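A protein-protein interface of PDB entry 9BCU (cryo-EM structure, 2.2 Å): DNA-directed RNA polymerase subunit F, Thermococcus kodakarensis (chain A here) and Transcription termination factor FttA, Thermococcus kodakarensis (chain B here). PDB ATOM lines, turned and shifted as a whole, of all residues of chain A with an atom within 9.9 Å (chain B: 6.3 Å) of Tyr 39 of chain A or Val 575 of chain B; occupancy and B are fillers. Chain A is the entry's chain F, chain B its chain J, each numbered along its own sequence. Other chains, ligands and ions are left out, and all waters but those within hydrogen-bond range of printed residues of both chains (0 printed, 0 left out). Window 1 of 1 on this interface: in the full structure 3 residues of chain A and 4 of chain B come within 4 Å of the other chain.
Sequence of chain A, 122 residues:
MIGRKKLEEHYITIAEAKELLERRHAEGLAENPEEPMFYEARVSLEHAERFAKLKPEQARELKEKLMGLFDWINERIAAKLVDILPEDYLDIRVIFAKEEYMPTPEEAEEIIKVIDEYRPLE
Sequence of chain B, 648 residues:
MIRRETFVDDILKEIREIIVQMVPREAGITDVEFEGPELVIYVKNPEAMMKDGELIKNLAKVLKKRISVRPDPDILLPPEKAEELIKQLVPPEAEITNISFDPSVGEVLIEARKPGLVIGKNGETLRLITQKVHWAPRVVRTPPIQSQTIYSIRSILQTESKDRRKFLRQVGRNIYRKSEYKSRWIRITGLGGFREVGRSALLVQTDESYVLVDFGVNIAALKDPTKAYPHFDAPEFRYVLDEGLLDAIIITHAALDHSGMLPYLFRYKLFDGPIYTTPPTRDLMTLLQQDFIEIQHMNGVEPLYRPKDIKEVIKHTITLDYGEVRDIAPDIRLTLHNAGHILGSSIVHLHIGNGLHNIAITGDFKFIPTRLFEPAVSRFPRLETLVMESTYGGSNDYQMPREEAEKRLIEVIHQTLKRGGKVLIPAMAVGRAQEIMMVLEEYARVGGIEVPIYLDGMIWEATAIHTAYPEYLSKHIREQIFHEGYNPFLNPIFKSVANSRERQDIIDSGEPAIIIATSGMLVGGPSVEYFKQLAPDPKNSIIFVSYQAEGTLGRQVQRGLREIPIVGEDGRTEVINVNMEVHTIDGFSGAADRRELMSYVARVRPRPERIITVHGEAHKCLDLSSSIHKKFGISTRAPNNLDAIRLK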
ATOM      1  N   LEU A  21     -22.490   6.723 -15.718  1.00  0.00           N
ATOM      2  CA  LEU A  21     -22.782   8.147 -15.822  1.00  0.00           C
ATOM      3  C   LEU A  21     -24.119   8.495 -15.182  1.00  0.00           C
ATOM      4  O   LEU A  21     -24.256   9.574 -14.602  1.00  0.00           O
ATOM      5  CB  LEU A  21     -22.757   8.583 -17.287  1.00  0.00           C
ATOM      6  CG  LEU A  21     -21.364   8.765 -17.894  1.00  0.00           C
ATOM      7  CD1 LEU A  21     -21.408   8.617 -19.407  1.00  0.00           C
ATOM      8  CD2 LEU A  21     -20.776  10.111 -17.500  1.00  0.00           C
ATOM      9  N   ARG A  24     -23.385   8.614 -11.501  1.00  0.00           N
ATOM     10  CA  ARG A  24     -22.685   9.850 -11.168  1.00  0.00           C
ATOM     11  C   ARG A  24     -23.615  11.056 -11.241  1.00  0.00           C
ATOM     12  O   ARG A  24     -23.487  11.993 -10.445  1.00  0.00           O
ATOM     13  CB  ARG A  24     -21.483  10.039 -12.090  1.00  0.00           C
ATOM     14  CG  ARG A  24     -20.195   9.470 -11.528  1.00  0.00           C
ATOM     15  CD  ARG A  24     -19.656  10.332 -10.398  1.00  0.00           C
ATOM     16  NE  ARG A  24     -19.303  11.672 -10.848  1.00  0.00           N
ATOM     17  CZ  ARG A  24     -19.747  12.790 -10.290  1.00  0.00           C
ATOM     18  NH1 ARG A  24     -20.571  12.767  -9.256  1.00  0.00           N
ATOM     19  NH2 ARG A  24     -19.355  13.961 -10.784  1.00  0.00           N
ATOM     20  N   HIS A  25     -24.553  11.053 -12.191  1.00  0.00           N
ATOM     21  CA  HIS A  25     -25.539  12.125 -12.273  1.00  0.00           C
ATOM     22  C   HIS A  25     -26.441  12.135 -11.047  1.00  0.00           C
ATOM     23  O   HIS A  25     -26.773  13.201 -10.520  1.00  0.00           O
ATOM     24  CB  HIS A  25     -26.365  11.977 -13.551  1.00  0.00           C
ATOM     25  CG  HIS A  25     -27.288  13.125 -13.813  1.00  0.00           C
ATOM     26  ND1 HIS A  25     -27.002  14.118 -14.726  1.00  0.00           N
ATOM     27  CD2 HIS A  25     -28.499  13.435 -13.290  1.00  0.00           C
ATOM     28  CE1 HIS A  25     -27.992  14.992 -14.750  1.00  0.00           C
ATOM     29  NE2 HIS A  25     -28.913  14.600 -13.887  1.00  0.00           N
ATOM     30  N   GLU A  35     -25.639  21.709 -10.438  1.00  0.00           N
ATOM     31  CA  GLU A  35     -24.873  21.133 -11.536  1.00  0.00           C
ATOM     32  C   GLU A  35     -24.362  19.762 -11.117  1.00  0.00           C
ATOM     33  O   GLU A  35     -23.530  19.678 -10.199  1.00  0.00           O
ATOM     34  CB  GLU A  35     -23.714  22.043 -11.915  1.00  0.00           C
ATOM     35  CG  GLU A  35     -23.178  21.815 -13.318  1.00  0.00           C
ATOM     36  CD  GLU A  35     -24.281  21.691 -14.350  1.00  0.00           C
ATOM     37  OE1 GLU A  35     -25.045  22.664 -14.526  1.00  0.00           O
ATOM     38  OE2 GLU A  35     -24.383  20.622 -14.986  1.00  0.00           O
ATOM     39  N   PRO A  36     -24.820  18.672 -11.739  1.00  0.00           N
ATOM     40  CA  PRO A  36     -24.339  17.346 -11.315  1.00  0.00           C
ATOM     41  C   PRO A  36     -22.898  17.080 -11.707  1.00  0.00           C
ATOM     42  O   PRO A  36     -22.121  16.575 -10.886  1.00  0.00           O
ATOM     43  CB  PRO A  36     -25.308  16.378 -12.012  1.00  0.00           C
ATOM     44  CG  PRO A  36     -26.435  17.233 -12.540  1.00  0.00           C
ATOM     45  CD  PRO A  36     -25.846  18.579 -12.787  1.00  0.00           C
ATOM     46  N   MET A  37     -22.514  17.404 -12.938  1.00  0.00           N
ATOM     47  CA  MET A  37     -21.155  17.178 -13.410  1.00  0.00           C
ATOM     48  C   MET A  37     -20.803  18.279 -14.404  1.00  0.00           C
ATOM     49  O   MET A  37     -21.548  19.249 -14.573  1.00  0.00           O
ATOM     50  CB  MET A  37     -21.018  15.779 -14.020  1.00  0.00           C
ATOM     51  CG  MET A  37     -22.228  15.329 -14.820  1.00  0.00           C
ATOM     52  SD  MET A  37     -22.501  13.552 -14.711  1.00  0.00           S
ATOM     53  CE  MET A  37     -23.796  13.338 -15.927  1.00  0.00           C
ATOM     54  N   PHE A  38     -19.662  18.126 -15.067  1.00  0.00           N
ATOM     55  CA  PHE A  38     -19.177  19.127 -16.004  1.00  0.00           C
ATOM     56  C   PHE A  38     -19.772  18.875 -17.388  1.00  0.00           C
ATOM     57  O   PHE A  38     -20.673  18.052 -17.565  1.00  0.00           O
ATOM     58  CB  PHE A  38     -17.649  19.138 -16.026  1.00  0.00           C
ATOM     59  CG  PHE A  38     -17.028  17.770 -16.044  1.00  0.00           C
ATOM     60  CD1 PHE A  38     -16.833  17.099 -17.239  1.00  0.00           C
ATOM     61  CD2 PHE A  38     -16.629  17.160 -14.866  1.00  0.00           C
ATOM     62  CE1 PHE A  38     -16.259  15.843 -17.258  1.00  0.00           C
ATOM     63  CE2 PHE A  38     -16.057  15.904 -14.880  1.00  0.00           C
ATOM     64  CZ  PHE A  38     -15.871  15.247 -16.079  1.00  0.00           C
ATOM     65  N   TYR A  39     -19.265  19.598 -18.391  1.00  0.00           N
ATOM     66  CA  TYR A  39     -19.831  19.520 -19.734  1.00  0.00           C
ATOM     67  C   TYR A  39     -19.557  18.169 -20.385  1.00  0.00           C
ATOM     68  O   TYR A  39     -20.445  17.590 -21.020  1.00  0.00           O
ATOM     69  CB  TYR A  39     -19.275  20.654 -20.595  1.00  0.00           C
ATOM     70  CG  TYR A  39     -19.787  20.671 -22.016  1.00  0.00           C
ATOM     71  CD1 TYR A  39     -21.077  21.093 -22.305  1.00  0.00           C
ATOM     72  CD2 TYR A  39     -18.976  20.273 -23.071  1.00  0.00           C
ATOM     73  CE1 TYR A  39     -21.548  21.112 -23.605  1.00  0.00           C
ATOM     74  CE2 TYR A  39     -19.437  20.290 -24.373  1.00  0.00           C
ATOM     75  CZ  TYR A  39     -20.724  20.712 -24.634  1.00  0.00           C
ATOM     76  OH  TYR A  39     -21.188  20.729 -25.929  1.00  0.00           O
ATOM     77  N   GLU A  40     -18.331  17.654 -20.241  1.00  0.00           N
ATOM     78  CA  GLU A  40     -17.956  16.424 -20.934  1.00  0.00           C
ATOM     79  C   GLU A  40     -18.736  15.222 -20.414  1.00  0.00           C
ATOM     80  O   GLU A  40     -19.173  14.377 -21.200  1.00  0.00           O
ATOM     81  CB  GLU A  40     -16.453  16.186 -20.803  1.00  0.00           C
ATOM     82  CG  GLU A  40     -15.647  16.656 -22.002  1.00  0.00           C
ATOM     83  CD  GLU A  40     -15.235  18.109 -21.891  1.00  0.00           C
ATOM     84  OE1 GLU A  40     -15.027  18.585 -20.755  1.00  0.00           O
ATOM     85  OE2 GLU A  40     -15.120  18.777 -22.940  1.00  0.00           O
ATOM     86  N   ALA A  41     -18.917  15.126 -19.094  1.00  0.00           N
ATOM     87  CA  ALA A  41     -19.663  14.004 -18.530  1.00  0.00           C
ATOM     88  C   ALA A  41     -21.127  14.038 -18.955  1.00  0.00           C
ATOM     89  O   ALA A  41     -21.702  13.000 -19.299  1.00  0.00           O
ATOM     90  CB  ALA A  41     -19.543  14.007 -17.007  1.00  0.00           C
ATOM     91  N   ARG A  42     -21.741  15.224 -18.938  1.00  0.00           N
ATOM     92  CA  ARG A  42     -23.127  15.355 -19.380  1.00  0.00           C
ATOM     93  C   ARG A  42     -23.269  15.013 -20.858  1.00  0.00           C
ATOM     94  O   ARG A  42     -24.226  14.338 -21.260  1.00  0.00           O
ATOM     95  CB  ARG A  42     -23.626  16.772 -19.100  1.00  0.00           C
ATOM     96  CG  ARG A  42     -24.809  17.209 -19.947  1.00  0.00           C
ATOM     97  CD  ARG A  42     -25.645  18.267 -19.225  1.00  0.00           C
ATOM     98  NE  ARG A  42     -25.145  19.638 -19.335  1.00  0.00           N
ATOM     99  CZ  ARG A  42     -24.816  20.273 -20.457  1.00  0.00           C
ATOM    100  NH1 ARG A  42     -25.039  19.747 -21.652  1.00  0.00           N
ATOM    101  NH2 ARG A  42     -24.282  21.487 -20.378  1.00  0.00           N
ATOM    102  N   VAL A  43     -22.318  15.463 -21.680  1.00  0.00           N
ATOM    103  CA  VAL A  43     -22.352  15.165 -23.109  1.00  0.00           C
ATOM    104  C   VAL A  43     -22.198  13.667 -23.348  1.00  0.00           C
ATOM    105  O   VAL A  43     -22.891  13.081 -24.189  1.00  0.00           O
ATOM    106  CB  VAL A  43     -21.269  15.984 -23.839  1.00  0.00           C
ATOM    107  CG1 VAL A  43     -20.888  15.338 -25.155  1.00  0.00           C
ATOM    108  CG2 VAL A  43     -21.752  17.406 -24.066  1.00  0.00           C
ATOM    109  N   SER A  44     -21.293  13.021 -22.605  1.00  0.00           N
ATOM    110  CA  SER A  44     -21.115  11.577 -22.728  1.00  0.00           C
ATOM    111  C   SER A  44     -22.373  10.827 -22.313  1.00  0.00           C
ATOM    112  O   SER A  44     -22.760   9.845 -22.959  1.00  0.00           O
ATOM    113  CB  SER A  44     -19.921  11.124 -21.890  1.00  0.00           C
ATOM    114  OG  SER A  44     -18.704  11.334 -22.581  1.00  0.00           O
ATOM    115  N   LEU A  45     -23.019  11.268 -21.228  1.00  0.00           N
ATOM    116  CA  LEU A  45     -24.261  10.633 -20.798  1.00  0.00           C
ATOM    117  C   LEU A  45     -25.353  10.789 -21.849  1.00  0.00           C
ATOM    118  O   LEU A  45     -26.091   9.838 -22.132  1.00  0.00           O
ATOM    119  CB  LEU A  45     -24.717  11.217 -19.461  1.00  0.00           C
ATOM    120  CG  LEU A  45     -26.095  10.766 -18.967  1.00  0.00           C
ATOM    121  CD1 LEU A  45     -26.126   9.261 -18.744  1.00  0.00           C
ATOM    122  CD2 LEU A  45     -26.490  11.507 -17.700  1.00  0.00           C
ATOM    123  N   GLU A  46     -25.465  11.981 -22.441  1.00  0.00           N
ATOM    124  CA  GLU A  46     -26.463  12.201 -23.485  1.00  0.00           C
ATOM    125  C   GLU A  46     -26.190  11.328 -24.704  1.00  0.00           C
ATOM    126  O   GLU A  46     -27.117  10.747 -25.280  1.00  0.00           O
ATOM    127  CB  GLU A  46     -26.496  13.677 -23.876  1.00  0.00           C
ATOM    128  CG  GLU A  46     -27.406  14.529 -23.007  1.00  0.00           C
ATOM    129  CD  GLU A  46     -27.270  16.010 -23.300  1.00  0.00           C
ATOM    130  OE1 GLU A  46     -27.093  16.369 -24.484  1.00  0.00           O
ATOM    131  OE2 GLU A  46     -27.341  16.815 -22.349  1.00  0.00           O
ATOM    132  N   HIS A  47     -24.922  11.223 -25.111  1.00  0.00           N
ATOM    133  CA  HIS A  47     -24.575  10.390 -26.258  1.00  0.00           C
ATOM    134  C   HIS A  47     -24.857   8.917 -25.983  1.00  0.00           C
ATOM    135  O   HIS A  47     -25.372   8.205 -26.854  1.00  0.00           O
ATOM    136  CB  HIS A  47     -23.106  10.595 -26.628  1.00  0.00           C
ATOM    137  CG  HIS A  47     -22.633   9.713 -27.742  1.00  0.00           C
ATOM    138  ND1 HIS A  47     -22.062   8.479 -27.523  1.00  0.00           N
ATOM    139  CD2 HIS A  47     -22.645   9.890 -29.084  1.00  0.00           C
ATOM    140  CE1 HIS A  47     -21.743   7.931 -28.683  1.00  0.00           C
ATOM    141  NE2 HIS A  47     -22.087   8.767 -29.646  1.00  0.00           N
ATOM    142  N   GLU B 563     -25.998  27.713 -24.969  1.00  0.00           N
ATOM    143  CA  GLU B 563     -24.831  27.362 -24.175  1.00  0.00           C
ATOM    144  C   GLU B 563     -23.626  27.200 -25.091  1.00  0.00           C
ATOM    145  O   GLU B 563     -23.749  26.703 -26.214  1.00  0.00           O
ATOM    146  CB  GLU B 563     -25.067  26.078 -23.366  1.00  0.00           C
ATOM    147  CG  GLU B 563     -25.406  24.855 -24.201  1.00  0.00           C
ATOM    148  CD  GLU B 563     -25.991  23.728 -23.373  1.00  0.00           C
ATOM    149  OE1 GLU B 563     -25.976  23.835 -22.128  1.00  0.00           O
ATOM    150  OE2 GLU B 563     -26.467  22.737 -23.965  1.00  0.00           O
ATOM    151  N   ILE B 564     -22.462  27.636 -24.607  1.00  0.00           N
ATOM    152  CA  ILE B 564     -21.224  27.584 -25.369  1.00  0.00           C
ATOM    153  C   ILE B 564     -20.137  26.991 -24.482  1.00  0.00           C
ATOM    154  O   ILE B 564     -19.830  27.551 -23.425  1.00  0.00           O
ATOM    155  CB  ILE B 564     -20.793  28.970 -25.884  1.00  0.00           C
ATOM    156  CG1 ILE B 564     -21.743  29.451 -26.982  1.00  0.00           C
ATOM    157  CG2 ILE B 564     -19.365  28.926 -26.400  1.00  0.00           C
ATOM    158  CD1 ILE B 564     -22.118  30.911 -26.868  1.00  0.00           C
ATOM    159  N   PRO B 565     -19.529  25.864 -24.854  1.00  0.00           N
ATOM    160  CA  PRO B 565     -18.445  25.302 -24.036  1.00  0.00           C
ATOM    161  C   PRO B 565     -17.128  26.015 -24.317  1.00  0.00           C
ATOM    162  O   PRO B 565     -16.700  26.131 -25.468  1.00  0.00           O
ATOM    163  CB  PRO B 565     -18.393  23.834 -24.472  1.00  0.00           C
ATOM    164  CG  PRO B 565     -18.944  23.828 -25.863  1.00  0.00           C
ATOM    165  CD  PRO B 565     -19.836  25.032 -26.031  1.00  0.00           C
ATOM    166  N   ILE B 566     -16.487  26.498 -23.252  1.00  0.00           N
ATOM    167  CA  ILE B 566     -15.220  27.206 -23.349  1.00  0.00           C
ATOM    168  C   ILE B 566     -14.249  26.622 -22.333  1.00  0.00           C
ATOM    169  O   ILE B 566     -14.641  25.962 -21.369  1.00  0.00           O
ATOM    170  CB  ILE B 566     -15.375  28.726 -23.123  1.00  0.00           C
ATOM    171  CG1 ILE B 566     -16.026  28.996 -21.767  1.00  0.00           C
ATOM    172  CG2 ILE B 566     -16.177  29.361 -24.250  1.00  0.00           C
ATOM    173  CD1 ILE B 566     -15.327  30.062 -20.956  1.00  0.00           C
ATOM    174  N   THR B 573     -13.467  22.388 -18.944  1.00  0.00           N
ATOM    175  CA  THR B 573     -14.481  22.995 -19.793  1.00  0.00           C
ATOM    176  C   THR B 573     -15.493  23.768 -18.954  1.00  0.00           C
ATOM    177  O   THR B 573     -15.944  23.298 -17.906  1.00  0.00           O
ATOM    178  CB  THR B 573     -15.195  21.925 -20.618  1.00  0.00           C
ATOM    179  OG1 THR B 573     -14.232  20.999 -21.137  1.00  0.00           O
ATOM    180  CG2 THR B 573     -15.953  22.559 -21.774  1.00  0.00           C
ATOM    181  N   GLU B 574     -15.845  24.960 -19.424  1.00  0.00           N
ATOM    182  CA  GLU B 574     -16.819  25.816 -18.764  1.00  0.00           C
ATOM    183  C   GLU B 574     -17.972  26.095 -19.716  1.00  0.00           C
ATOM    184  O   GLU B 574     -17.771  26.230 -20.927  1.00  0.00           O
ATOM    185  CB  GLU B 574     -16.182  27.133 -18.308  1.00  0.00           C
ATOM    186  CG  GLU B 574     -16.622  27.589 -16.927  1.00  0.00           C
ATOM    187  CD  GLU B 574     -16.477  29.085 -16.734  1.00  0.00           C
ATOM    188  OE1 GLU B 574     -15.972  29.759 -17.657  1.00  0.00           O
ATOM    189  OE2 GLU B 574     -16.866  29.589 -15.660  1.00  0.00           O
ATOM    190  N   VAL B 575     -19.179  26.183 -19.164  1.00  0.00           N
ATOM    191  CA  VAL B 575     -20.395  26.393 -19.941  1.00  0.00           C
ATOM    192  C   VAL B 575     -20.915  27.793 -19.655  1.00  0.00           C
ATOM    193  O   VAL B 575     -21.130  28.158 -18.492  1.00  0.00           O
ATOM    194  CB  VAL B 575     -21.462  25.333 -19.616  1.00  0.00           C
ATOM    195  CG1 VAL B 575     -22.726  25.589 -20.420  1.00  0.00           C
ATOM    196  CG2 VAL B 575     -20.922  23.939 -19.890  1.00  0.00           C
ATOM    197  N   ILE B 576     -21.115  28.574 -20.711  1.00  0.00           N
ATOM    198  CA  ILE B 576     -21.651  29.926 -20.608  1.00  0.00           C
ATOM    199  C   ILE B 576     -23.122  29.880 -20.994  1.00  0.00           C
ATOM    200  O   ILE B 576     -23.463  29.550 -22.136  1.00  0.00           O
ATOM    201  CB  ILE B 576     -20.878  30.907 -21.502  1.00  0.00           C
ATOM    202  CG1 ILE B 576     -19.401  30.940 -21.111  1.00  0.00           C
ATOM    203  CG2 ILE B 576     -21.486  32.298 -21.413  1.00  0.00           C
ATOM    204  CD1 ILE B 576     -18.537  31.708 -22.084  1.00  0.00           C
ATOM    205  N   ASN B 577     -23.995  30.217 -20.048  1.00  0.00           N
ATOM    206  CA  ASN B 577     -25.434  30.231 -20.285  1.00  0.00           C
ATOM    207  C   ASN B 577     -25.816  31.594 -20.850  1.00  0.00           C
ATOM    208  O   ASN B 577     -25.822  32.595 -20.128  1.00  0.00           O
ATOM    209  CB  ASN B 577     -26.196  29.930 -18.998  1.00  0.00           C
ATOM    210  CG  ASN B 577     -26.120  28.468 -18.606  1.00  0.00           C
ATOM    211  OD1 ASN B 577     -25.290  28.075 -17.787  1.00  0.00           O
ATOM    212  ND2 ASN B 577     -26.988  27.653 -19.193  1.00  0.00           N
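Tyr 39 of chain A touches Pro 565 of chain B.
CD1 of Tyr 39 of chain A touches CG2 of Val 575 of chain B, 3.7 Å away.
Printed residues of chain A that touch a printed residue of chain B: Tyr 39, Glu 40 and Arg 42.
Along chain A the printed residues that touch a printed residue of chain B span positions 39 to 42.
Printed residues of chain B that touch a printed residue of chain A: Glu 563, Pro 565, Thr 573 and Val 575.
Hydrophobic or aromatic side chains of chain B within 4 Å of the printed part of chain A: Pro 565 and Val 575.
Among the printed residues, 4 pairs touch across the chains.
Printed residues of chain B within 4 Å of Tyr 39 of chain A: Pro 565 (3.7 Å) and Val 575 (3.7 Å).
Glu 574 of chain B touches none of the printed residues of chain A.
Ile 576 of chain B touches none of the printed residues of chain A.
Of the printed residues of chain A, Pro 565 of chain B touches Tyr 39 (3.7 Å).
Of the printed residues of chain B, Arg 42 of chain A touches Glu 563 (3.4 Å).
Of the printed residues of chain B, Glu 40 of chain A touches Thr 573 (2.6 Å).
Of the printed residues of chain A, Glu 563 of chain B touches Arg 42 (3.4 Å).
Printed residues of chain A within 4 Å of Thr 573 of chain B: Glu 40 (2.6 Å).
Arg 24 of chain A touches none of the printed residues of chain B.
Ser 44 of chain A touches none of the printed residues of chain B.
The nearest printed residue of chain B that does not touch Tyr 39 of chain A is Thr 573 of chain B (4.01 Å).
The nearest residue of chain A that does not touch Val 575 of chain B is Arg 42 of chain A (4.2 Å).
The nearest printed residue of chain A that does not touch Thr 573 of chain B is Tyr 39 of chain A (4.01 Å).
The side-chain carboxylate of Glu 563 of chain B is in salt-bridge range of the guanidinium group of Arg 42 of chain A, at 3.4 Å.
The side-chain hydroxyl of Thr 573 of chain B sits at hydrogen-bond distance from the side-chain carboxylate of Glu 40 of chain A (2.6 Å).
O of Glu 40 of chain A is in hydrogen-bond range of OG of Ser 44 of chain A.
The side-chain carboxylate (OE2) of Glu 46 of chain A is in salt-bridge range of the guanidinium group (NH1) of Arg 42 of chain A (3.8 Å).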
